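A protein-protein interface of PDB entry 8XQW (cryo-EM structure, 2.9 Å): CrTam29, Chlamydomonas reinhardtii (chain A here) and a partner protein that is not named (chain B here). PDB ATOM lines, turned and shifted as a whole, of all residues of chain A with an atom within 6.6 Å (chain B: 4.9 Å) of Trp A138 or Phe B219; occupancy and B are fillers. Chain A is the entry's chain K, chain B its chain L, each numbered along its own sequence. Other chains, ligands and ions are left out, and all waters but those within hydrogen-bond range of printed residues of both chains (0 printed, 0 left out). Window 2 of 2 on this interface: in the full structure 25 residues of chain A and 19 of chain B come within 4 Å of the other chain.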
ATOM      1  N   LYS A 136     -26.190 -16.514  -2.615  1.00  0.00           N
ATOM      2  CA  LYS A 136     -25.068 -15.595  -2.528  1.00  0.00           C
ATOM      3  C   LYS A 136     -24.453 -15.302  -3.885  1.00  0.00           C
ATOM      4  O   LYS A 136     -23.290 -14.907  -3.944  1.00  0.00           O
ATOM      5  CB  LYS A 136     -23.998 -16.151  -1.601  1.00  0.00           C
ATOM      6  CG  LYS A 136     -24.495 -16.475  -0.239  1.00  0.00           C
ATOM      7  CD  LYS A 136     -23.457 -17.227   0.505  1.00  0.00           C
ATOM      8  CE  LYS A 136     -23.417 -16.810   1.929  1.00  0.00           C
ATOM      9  NZ  LYS A 136     -22.201 -17.335   2.581  1.00  0.00           N
ATOM     10  N   ARG A 137     -25.183 -15.499  -4.970  1.00  0.00           N
ATOM     11  CA  ARG A 137     -24.666 -15.155  -6.278  1.00  0.00           C
ATOM     12  C   ARG A 137     -24.789 -13.663  -6.500  1.00  0.00           C
ATOM     13  O   ARG A 137     -25.836 -13.078  -6.232  1.00  0.00           O
ATOM     14  CB  ARG A 137     -25.430 -15.890  -7.360  1.00  0.00           C
ATOM     15  CG  ARG A 137     -25.079 -17.314  -7.511  1.00  0.00           C
ATOM     16  CD  ARG A 137     -25.991 -17.950  -8.500  1.00  0.00           C
ATOM     17  NE  ARG A 137     -25.637 -17.579  -9.855  1.00  0.00           N
ATOM     18  CZ  ARG A 137     -26.449 -16.932 -10.675  1.00  0.00           C
ATOM     19  NH1 ARG A 137     -26.050 -16.629 -11.891  1.00  0.00           N
ATOM     20  NH2 ARG A 137     -27.651 -16.589 -10.274  1.00  0.00           N
ATOM     21  N   TRP A 138     -23.730 -13.045  -6.998  1.00  0.00           N
ATOM     22  CA  TRP A 138     -23.751 -11.633  -7.340  1.00  0.00           C
ATOM     23  C   TRP A 138     -24.119 -11.527  -8.808  1.00  0.00           C
ATOM     24  O   TRP A 138     -23.378 -11.987  -9.672  1.00  0.00           O
ATOM     25  CB  TRP A 138     -22.404 -10.995  -7.038  1.00  0.00           C
ATOM     26  CG  TRP A 138     -22.342  -9.519  -7.224  1.00  0.00           C
ATOM     27  CD1 TRP A 138     -23.368  -8.641  -7.175  1.00  0.00           C
ATOM     28  CD2 TRP A 138     -21.176  -8.754  -7.486  1.00  0.00           C
ATOM     29  NE1 TRP A 138     -22.918  -7.374  -7.400  1.00  0.00           N
ATOM     30  CE2 TRP A 138     -21.568  -7.423  -7.596  1.00  0.00           C
ATOM     31  CE3 TRP A 138     -19.835  -9.071  -7.649  1.00  0.00           C
ATOM     32  CZ2 TRP A 138     -20.668  -6.413  -7.848  1.00  0.00           C
ATOM     33  CZ3 TRP A 138     -18.952  -8.072  -7.901  1.00  0.00           C
ATOM     34  CH2 TRP A 138     -19.365  -6.762  -8.001  1.00  0.00           C
ATOM     35  N   THR A 139     -25.283 -10.957  -9.089  1.00  0.00           N
ATOM     36  CA  THR A 139     -25.788 -10.791 -10.438  1.00  0.00           C
ATOM     37  C   THR A 139     -26.328  -9.382 -10.571  1.00  0.00           C
ATOM     38  O   THR A 139     -26.498  -8.680  -9.584  1.00  0.00           O
ATOM     39  CB  THR A 139     -26.881 -11.803 -10.756  1.00  0.00           C
ATOM     40  OG1 THR A 139     -27.891 -11.741  -9.756  1.00  0.00           O
ATOM     41  CG2 THR A 139     -26.320 -13.180 -10.767  1.00  0.00           C
ATOM     42  N   LEU A 140     -26.625  -8.969 -11.800  1.00  0.00           N
ATOM     43  CA  LEU A 140     -27.076  -7.602 -12.017  1.00  0.00           C
ATOM     44  C   LEU A 140     -28.462  -7.356 -11.452  1.00  0.00           C
ATOM     45  O   LEU A 140     -28.794  -6.216 -11.137  1.00  0.00           O
ATOM     46  CB  LEU A 140     -27.072  -7.258 -13.497  1.00  0.00           C
ATOM     47  CG  LEU A 140     -25.713  -7.176 -14.176  1.00  0.00           C
ATOM     48  CD1 LEU A 140     -25.870  -7.258 -15.661  1.00  0.00           C
ATOM     49  CD2 LEU A 140     -25.038  -5.895 -13.814  1.00  0.00           C
ATOM     50  N   PHE A 141     -29.296  -8.381 -11.340  1.00  0.00           N
ATOM     51  CA  PHE A 141     -30.595  -8.166 -10.724  1.00  0.00           C
ATOM     52  C   PHE A 141     -30.458  -7.925  -9.235  1.00  0.00           C
ATOM     53  O   PHE A 141     -31.204  -7.136  -8.659  1.00  0.00           O
ATOM     54  CB  PHE A 141     -31.513  -9.351 -10.972  1.00  0.00           C
ATOM     55  CG  PHE A 141     -32.721  -9.370 -10.084  1.00  0.00           C
ATOM     56  CD1 PHE A 141     -33.810  -8.583 -10.364  1.00  0.00           C
ATOM     57  CD2 PHE A 141     -32.769 -10.174  -8.967  1.00  0.00           C
ATOM     58  CE1 PHE A 141     -34.912  -8.592  -9.550  1.00  0.00           C
ATOM     59  CE2 PHE A 141     -33.873 -10.174  -8.153  1.00  0.00           C
ATOM     60  CZ  PHE A 141     -34.941  -9.390  -8.453  1.00  0.00           C
ATOM     61  N   SER A 142     -29.516  -8.597  -8.590  1.00  0.00           N
ATOM     62  CA  SER A 142     -29.407  -8.505  -7.148  1.00  0.00           C
ATOM     63  C   SER A 142     -28.788  -7.207  -6.675  1.00  0.00           C
ATOM     64  O   SER A 142     -29.081  -6.777  -5.559  1.00  0.00           O
ATOM     65  CB  SER A 142     -28.595  -9.663  -6.613  1.00  0.00           C
ATOM     66  OG  SER A 142     -27.231  -9.391  -6.766  1.00  0.00           O
ATOM     67  N   THR A 143     -27.963  -6.552  -7.482  1.00  0.00           N
ATOM     68  CA  THR A 143     -27.428  -5.282  -7.021  1.00  0.00           C
ATOM     69  C   THR A 143     -28.429  -4.143  -7.126  1.00  0.00           C
ATOM     70  O   THR A 143     -28.105  -3.031  -6.717  1.00  0.00           O
ATOM     71  CB  THR A 143     -26.149  -4.910  -7.767  1.00  0.00           C
ATOM     72  OG1 THR A 143     -26.347  -3.686  -8.455  1.00  0.00           O
ATOM     73  CG2 THR A 143     -25.783  -5.920  -8.754  1.00  0.00           C
ATOM     74  N   PHE A 252     -27.483 -15.796 -15.719  1.00  0.00           N
ATOM     75  CA  PHE A 252     -26.050 -15.618 -15.913  1.00  0.00           C
ATOM     76  C   PHE A 252     -25.645 -14.476 -15.010  1.00  0.00           C
ATOM     77  O   PHE A 252     -26.220 -14.321 -13.937  1.00  0.00           O
ATOM     78  CB  PHE A 252     -25.690 -15.386 -17.376  1.00  0.00           C
ATOM     79  CG  PHE A 252     -25.503 -16.660 -18.149  1.00  0.00           C
ATOM     80  CD1 PHE A 252     -24.676 -17.654 -17.677  1.00  0.00           C
ATOM     81  CD2 PHE A 252     -26.192 -16.882 -19.316  1.00  0.00           C
ATOM     82  CE1 PHE A 252     -24.528 -18.824 -18.368  1.00  0.00           C
ATOM     83  CE2 PHE A 252     -26.043 -18.052 -20.004  1.00  0.00           C
ATOM     84  CZ  PHE A 252     -25.214 -19.018 -19.532  1.00  0.00           C
ATOM     85  N   TRP A 253     -24.625 -13.716 -15.374  1.00  0.00           N
ATOM     86  CA  TRP A 253     -24.433 -12.429 -14.719  1.00  0.00           C
ATOM     87  C   TRP A 253     -25.706 -11.594 -14.684  1.00  0.00           C
ATOM     88  O   TRP A 253     -25.775 -10.623 -13.937  1.00  0.00           O
ATOM     89  CB  TRP A 253     -23.347 -11.620 -15.419  1.00  0.00           C
ATOM     90  CG  TRP A 253     -22.278 -12.444 -15.984  1.00  0.00           C
ATOM     91  CD1 TRP A 253     -21.170 -12.882 -15.346  1.00  0.00           C
ATOM     92  CD2 TRP A 253     -22.204 -12.939 -17.315  1.00  0.00           C
ATOM     93  NE1 TRP A 253     -20.405 -13.631 -16.192  1.00  0.00           N
ATOM     94  CE2 TRP A 253     -21.019 -13.683 -17.412  1.00  0.00           C
ATOM     95  CE3 TRP A 253     -23.025 -12.829 -18.435  1.00  0.00           C
ATOM     96  CZ2 TRP A 253     -20.635 -14.315 -18.584  1.00  0.00           C
ATOM     97  CZ3 TRP A 253     -22.644 -13.456 -19.593  1.00  0.00           C
ATOM     98  CH2 TRP A 253     -21.460 -14.190 -19.661  1.00  0.00           C
ATOM     99  N   ASN B 215     -21.539  -8.874  -1.373  1.00  0.00           N
ATOM    100  CA  ASN B 215     -20.973  -8.338  -2.601  1.00  0.00           C
ATOM    101  C   ASN B 215     -21.657  -7.042  -2.994  1.00  0.00           C
ATOM    102  O   ASN B 215     -21.002  -6.077  -3.388  1.00  0.00           O
ATOM    103  CB  ASN B 215     -21.100  -9.353  -3.722  1.00  0.00           C
ATOM    104  CG  ASN B 215     -20.410 -10.635  -3.421  1.00  0.00           C
ATOM    105  OD1 ASN B 215     -19.224 -10.777  -3.644  1.00  0.00           O
ATOM    106  ND2 ASN B 215     -21.154 -11.591  -2.917  1.00  0.00           N
ATOM    107  N   GLU B 216     -22.978  -7.003  -2.905  1.00  0.00           N
ATOM    108  CA  GLU B 216     -23.692  -5.798  -3.286  1.00  0.00           C
ATOM    109  C   GLU B 216     -23.448  -4.675  -2.302  1.00  0.00           C
ATOM    110  O   GLU B 216     -23.412  -3.508  -2.689  1.00  0.00           O
ATOM    111  CB  GLU B 216     -25.174  -6.097  -3.402  1.00  0.00           C
ATOM    112  CG  GLU B 216     -25.485  -7.143  -4.418  1.00  0.00           C
ATOM    113  CD  GLU B 216     -25.418  -8.531  -3.863  1.00  0.00           C
ATOM    114  OE1 GLU B 216     -24.964  -8.674  -2.727  1.00  0.00           O
ATOM    115  OE2 GLU B 216     -25.821  -9.485  -4.545  1.00  0.00           O
ATOM    116  N   ARG B 217     -23.271  -5.002  -1.035  1.00  0.00           N
ATOM    117  CA  ARG B 217     -22.962  -3.980  -0.051  1.00  0.00           C
ATOM    118  C   ARG B 217     -21.619  -3.342  -0.348  1.00  0.00           C
ATOM    119  O   ARG B 217     -21.492  -2.117  -0.346  1.00  0.00           O
ATOM    120  CB  ARG B 217     -22.979  -4.600   1.333  1.00  0.00           C
ATOM    121  CG  ARG B 217     -23.098  -3.648   2.469  1.00  0.00           C
ATOM    122  CD  ARG B 217     -22.975  -4.414   3.743  1.00  0.00           C
ATOM    123  NE  ARG B 217     -22.719  -3.554   4.884  1.00  0.00           N
ATOM    124  CZ  ARG B 217     -22.380  -4.001   6.083  1.00  0.00           C
ATOM    125  NH1 ARG B 217     -22.260  -5.296   6.288  1.00  0.00           N
ATOM    126  NH2 ARG B 217     -22.167  -3.160   7.072  1.00  0.00           N
ATOM    127  N   TRP B 218     -20.600  -4.154  -0.623  1.00  0.00           N
ATOM    128  CA  TRP B 218     -19.316  -3.560  -0.964  1.00  0.00           C
ATOM    129  C   TRP B 218     -19.390  -2.783  -2.260  1.00  0.00           C
ATOM    130  O   TRP B 218     -18.764  -1.734  -2.378  1.00  0.00           O
ATOM    131  CB  TRP B 218     -18.239  -4.624  -1.058  1.00  0.00           C
ATOM    132  CG  TRP B 218     -16.868  -4.087  -1.239  1.00  0.00           C
ATOM    133  CD1 TRP B 218     -16.028  -3.678  -0.273  1.00  0.00           C
ATOM    134  CD2 TRP B 218     -16.170  -3.921  -2.469  1.00  0.00           C
ATOM    135  NE1 TRP B 218     -14.852  -3.261  -0.812  1.00  0.00           N
ATOM    136  CE2 TRP B 218     -14.917  -3.406  -2.167  1.00  0.00           C
ATOM    137  CE3 TRP B 218     -16.490  -4.159  -3.800  1.00  0.00           C
ATOM    138  CZ2 TRP B 218     -13.989  -3.118  -3.138  1.00  0.00           C
ATOM    139  CZ3 TRP B 218     -15.571  -3.882  -4.752  1.00  0.00           C
ATOM    140  CH2 TRP B 218     -14.337  -3.367  -4.423  1.00  0.00           C
ATOM    141  N   PHE B 219     -20.155  -3.258  -3.237  1.00  0.00           N
ATOM    142  CA  PHE B 219     -20.254  -2.528  -4.491  1.00  0.00           C
ATOM    143  C   PHE B 219     -20.857  -1.154  -4.275  1.00  0.00           C
ATOM    144  O   PHE B 219     -20.312  -0.148  -4.725  1.00  0.00           O
ATOM    145  CB  PHE B 219     -21.077  -3.312  -5.493  1.00  0.00           C
ATOM    146  CG  PHE B 219     -21.349  -2.567  -6.748  1.00  0.00           C
ATOM    147  CD1 PHE B 219     -20.372  -2.405  -7.688  1.00  0.00           C
ATOM    148  CD2 PHE B 219     -22.584  -2.038  -6.995  1.00  0.00           C
ATOM    149  CE1 PHE B 219     -20.626  -1.721  -8.830  1.00  0.00           C
ATOM    150  CE2 PHE B 219     -22.830  -1.353  -8.135  1.00  0.00           C
ATOM    151  CZ  PHE B 219     -21.857  -1.201  -9.054  1.00  0.00           C
ATOM    152  N   TRP B 220     -21.978  -1.084  -3.575  1.00  0.00           N
ATOM    153  CA  TRP B 220     -22.616   0.206  -3.390  1.00  0.00           C
ATOM    154  C   TRP B 220     -21.894   1.091  -2.395  1.00  0.00           C
ATOM    155  O   TRP B 220     -22.123   2.298  -2.401  1.00  0.00           O
ATOM    156  CB  TRP B 220     -24.063   0.018  -2.961  1.00  0.00           C
ATOM    157  CG  TRP B 220     -24.942  -0.349  -4.084  1.00  0.00           C
ATOM    158  CD1 TRP B 220     -25.595  -1.514  -4.248  1.00  0.00           C
ATOM    159  CD2 TRP B 220     -25.256   0.449  -5.220  1.00  0.00           C
ATOM    160  NE1 TRP B 220     -26.298  -1.502  -5.413  1.00  0.00           N
ATOM    161  CE2 TRP B 220     -26.105  -0.301  -6.030  1.00  0.00           C
ATOM    162  CE3 TRP B 220     -24.895   1.730  -5.632  1.00  0.00           C
ATOM    163  CZ2 TRP B 220     -26.603   0.183  -7.221  1.00  0.00           C
ATOM    164  CZ3 TRP B 220     -25.390   2.203  -6.804  1.00  0.00           C
ATOM    165  CH2 TRP B 220     -26.230   1.434  -7.590  1.00  0.00           C
ATOM    166  N   GLU B 221     -21.019   0.551  -1.558  1.00  0.00           N
ATOM    167  CA  GLU B 221     -20.350   1.409  -0.591  1.00  0.00           C
ATOM    168  C   GLU B 221     -18.969   1.861  -1.023  1.00  0.00           C
ATOM    169  O   GLU B 221     -18.551   2.956  -0.648  1.00  0.00           O
ATOM    170  CB  GLU B 221     -20.222   0.705   0.753  1.00  0.00           C
ATOM    171  CG  GLU B 221     -21.529   0.426   1.429  1.00  0.00           C
ATOM    172  CD  GLU B 221     -22.044   1.611   2.194  1.00  0.00           C
ATOM    173  OE1 GLU B 221     -21.217   2.429   2.637  1.00  0.00           O
ATOM    174  OE2 GLU B 221     -23.274   1.727   2.351  1.00  0.00           O
ATOM    175  N   VAL B 222     -18.237   1.063  -1.790  1.00  0.00           N
ATOM    176  CA  VAL B 222     -16.827   1.346  -2.018  1.00  0.00           C
ATOM    177  C   VAL B 222     -16.506   1.481  -3.498  1.00  0.00           C
ATOM    178  O   VAL B 222     -15.507   2.096  -3.872  1.00  0.00           O
ATOM    179  CB  VAL B 222     -15.966   0.259  -1.362  1.00  0.00           C
ATOM    180  CG1 VAL B 222     -14.523   0.508  -1.606  1.00  0.00           C
ATOM    181  CG2 VAL B 222     -16.211   0.238   0.111  1.00  0.00           C
ATOM    182  N   PHE B 223     -17.350   0.949  -4.360  1.00  0.00           N
ATOM    183  CA  PHE B 223     -16.991   0.847  -5.762  1.00  0.00           C
ATOM    184  C   PHE B 223     -17.855   1.668  -6.697  1.00  0.00           C
ATOM    185  O   PHE B 223     -17.375   2.081  -7.739  1.00  0.00           O
ATOM    186  CB  PHE B 223     -17.048  -0.611  -6.195  1.00  0.00           C
ATOM    187  CG  PHE B 223     -16.409  -0.875  -7.505  1.00  0.00           C
ATOM    188  CD1 PHE B 223     -15.067  -1.101  -7.587  1.00  0.00           C
ATOM    189  CD2 PHE B 223     -17.152  -0.921  -8.650  1.00  0.00           C
ATOM    190  CE1 PHE B 223     -14.485  -1.343  -8.785  1.00  0.00           C
ATOM    191  CE2 PHE B 223     -16.567  -1.163  -9.844  1.00  0.00           C
ATOM    192  CZ  PHE B 223     -15.238  -1.379  -9.912  1.00  0.00           C
ATOM    193  N   ALA B 224     -19.119   1.920  -6.377  1.00  0.00           N
ATOM    194  CA  ALA B 224     -20.003   2.507  -7.374  1.00  0.00           C
ATOM    195  C   ALA B 224     -19.531   3.885  -7.794  1.00  0.00           C
ATOM    196  O   ALA B 224     -19.268   4.123  -8.972  1.00  0.00           O
ATOM    197  CB  ALA B 224     -21.427   2.578  -6.846  1.00  0.00           C
ATOM    198  N   LEU B 228     -16.253   3.819 -10.523  1.00  0.00           N
ATOM    199  CA  LEU B 228     -17.014   3.600 -11.745  1.00  0.00           C
ATOM    200  C   LEU B 228     -17.575   4.889 -12.327  1.00  0.00           C
ATOM    201  O   LEU B 228     -17.420   5.125 -13.523  1.00  0.00           O
ATOM    202  CB  LEU B 228     -18.131   2.593 -11.484  1.00  0.00           C
ATOM    203  CG  LEU B 228     -18.972   2.182 -12.680  1.00  0.00           C
ATOM    204  CD1 LEU B 228     -18.107   1.586 -13.738  1.00  0.00           C
ATOM    205  CD2 LEU B 228     -19.993   1.189 -12.233  1.00  0.00           C
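The side-chain hydroxyl of Ser A142 sits at hydrogen-bond distance from the side-chain carboxylate of Glu B216, 2.6 Å away.
O of Thr A143 sits at hydrogen-bond distance from NE1 of Trp B220, at 2.7 Å.
The guanidinium group (NH1) of Arg A137 lies within hydrogen-bond range of the backbone carbonyl oxygen (O) of Phe A252, 3.1 Å away.
The side-chain hydroxyl (OG) of Ser A142 lies within hydrogen-bond range of the backbone carbonyl oxygen (O) of Thr A139 (3.0 Å).
The backbone carbonyl oxygen (O) of Phe B219 lies within hydrogen-bond range of the backbone NH (N) of Ala B224 (2.9 Å).
Glu B216 touches Arg A137 (OE2 to O, 3.97 Å).
Trp A138 touches Asn B215.
Trp A138 touches Glu B216 (CD1 to OE2, 3.7 Å).
Phe B219 touches Trp A138 (CB to CZ2, 3.9 Å).
Glu B216 touches Thr A143 (CG to CA, 3.7 Å).
Printed residues of chain B within 4 Å of Arg A137: Glu B216 (3.97 Å).
Of chain B, only Asn B215 (3.7 Å), Glu B216 (3.7 Å) and Phe B219 (3.9 Å) come within 4 Å of Trp A138.
Phe A141 touches none of the printed residues of chain B.
Of the printed residues of chain B, Ser A142 touches Glu B216 (2.6 Å).
Of the printed residues of chain B, Thr A143 touches Glu B216 (3.7 Å) and Trp B220 (2.7 Å).
Of chain A, only Trp A138 (3.9 Å) comes within 4 Å of Phe B219.
Printed residues of chain A within 4 Å of Trp B220: Thr A143.
Ala B224 touches none of the printed residues of chain A.
The nearest printed residue of chain B that does not touch Trp A138 is Trp B218 (5.7 Å).
The nearest printed residue of chain B that does not touch Thr A143 is Phe B219 (4.2 Å).
Of the 11 printed residues of chain B, 4 touch a printed residue of chain A.
Of the 10 printed residues of chain A, 4 touch a printed residue of chain B.
Among the printed residues, no Asp or Glu carboxylate lies within 4 Å of a Lys or Arg side-chain nitrogen of the other chain.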
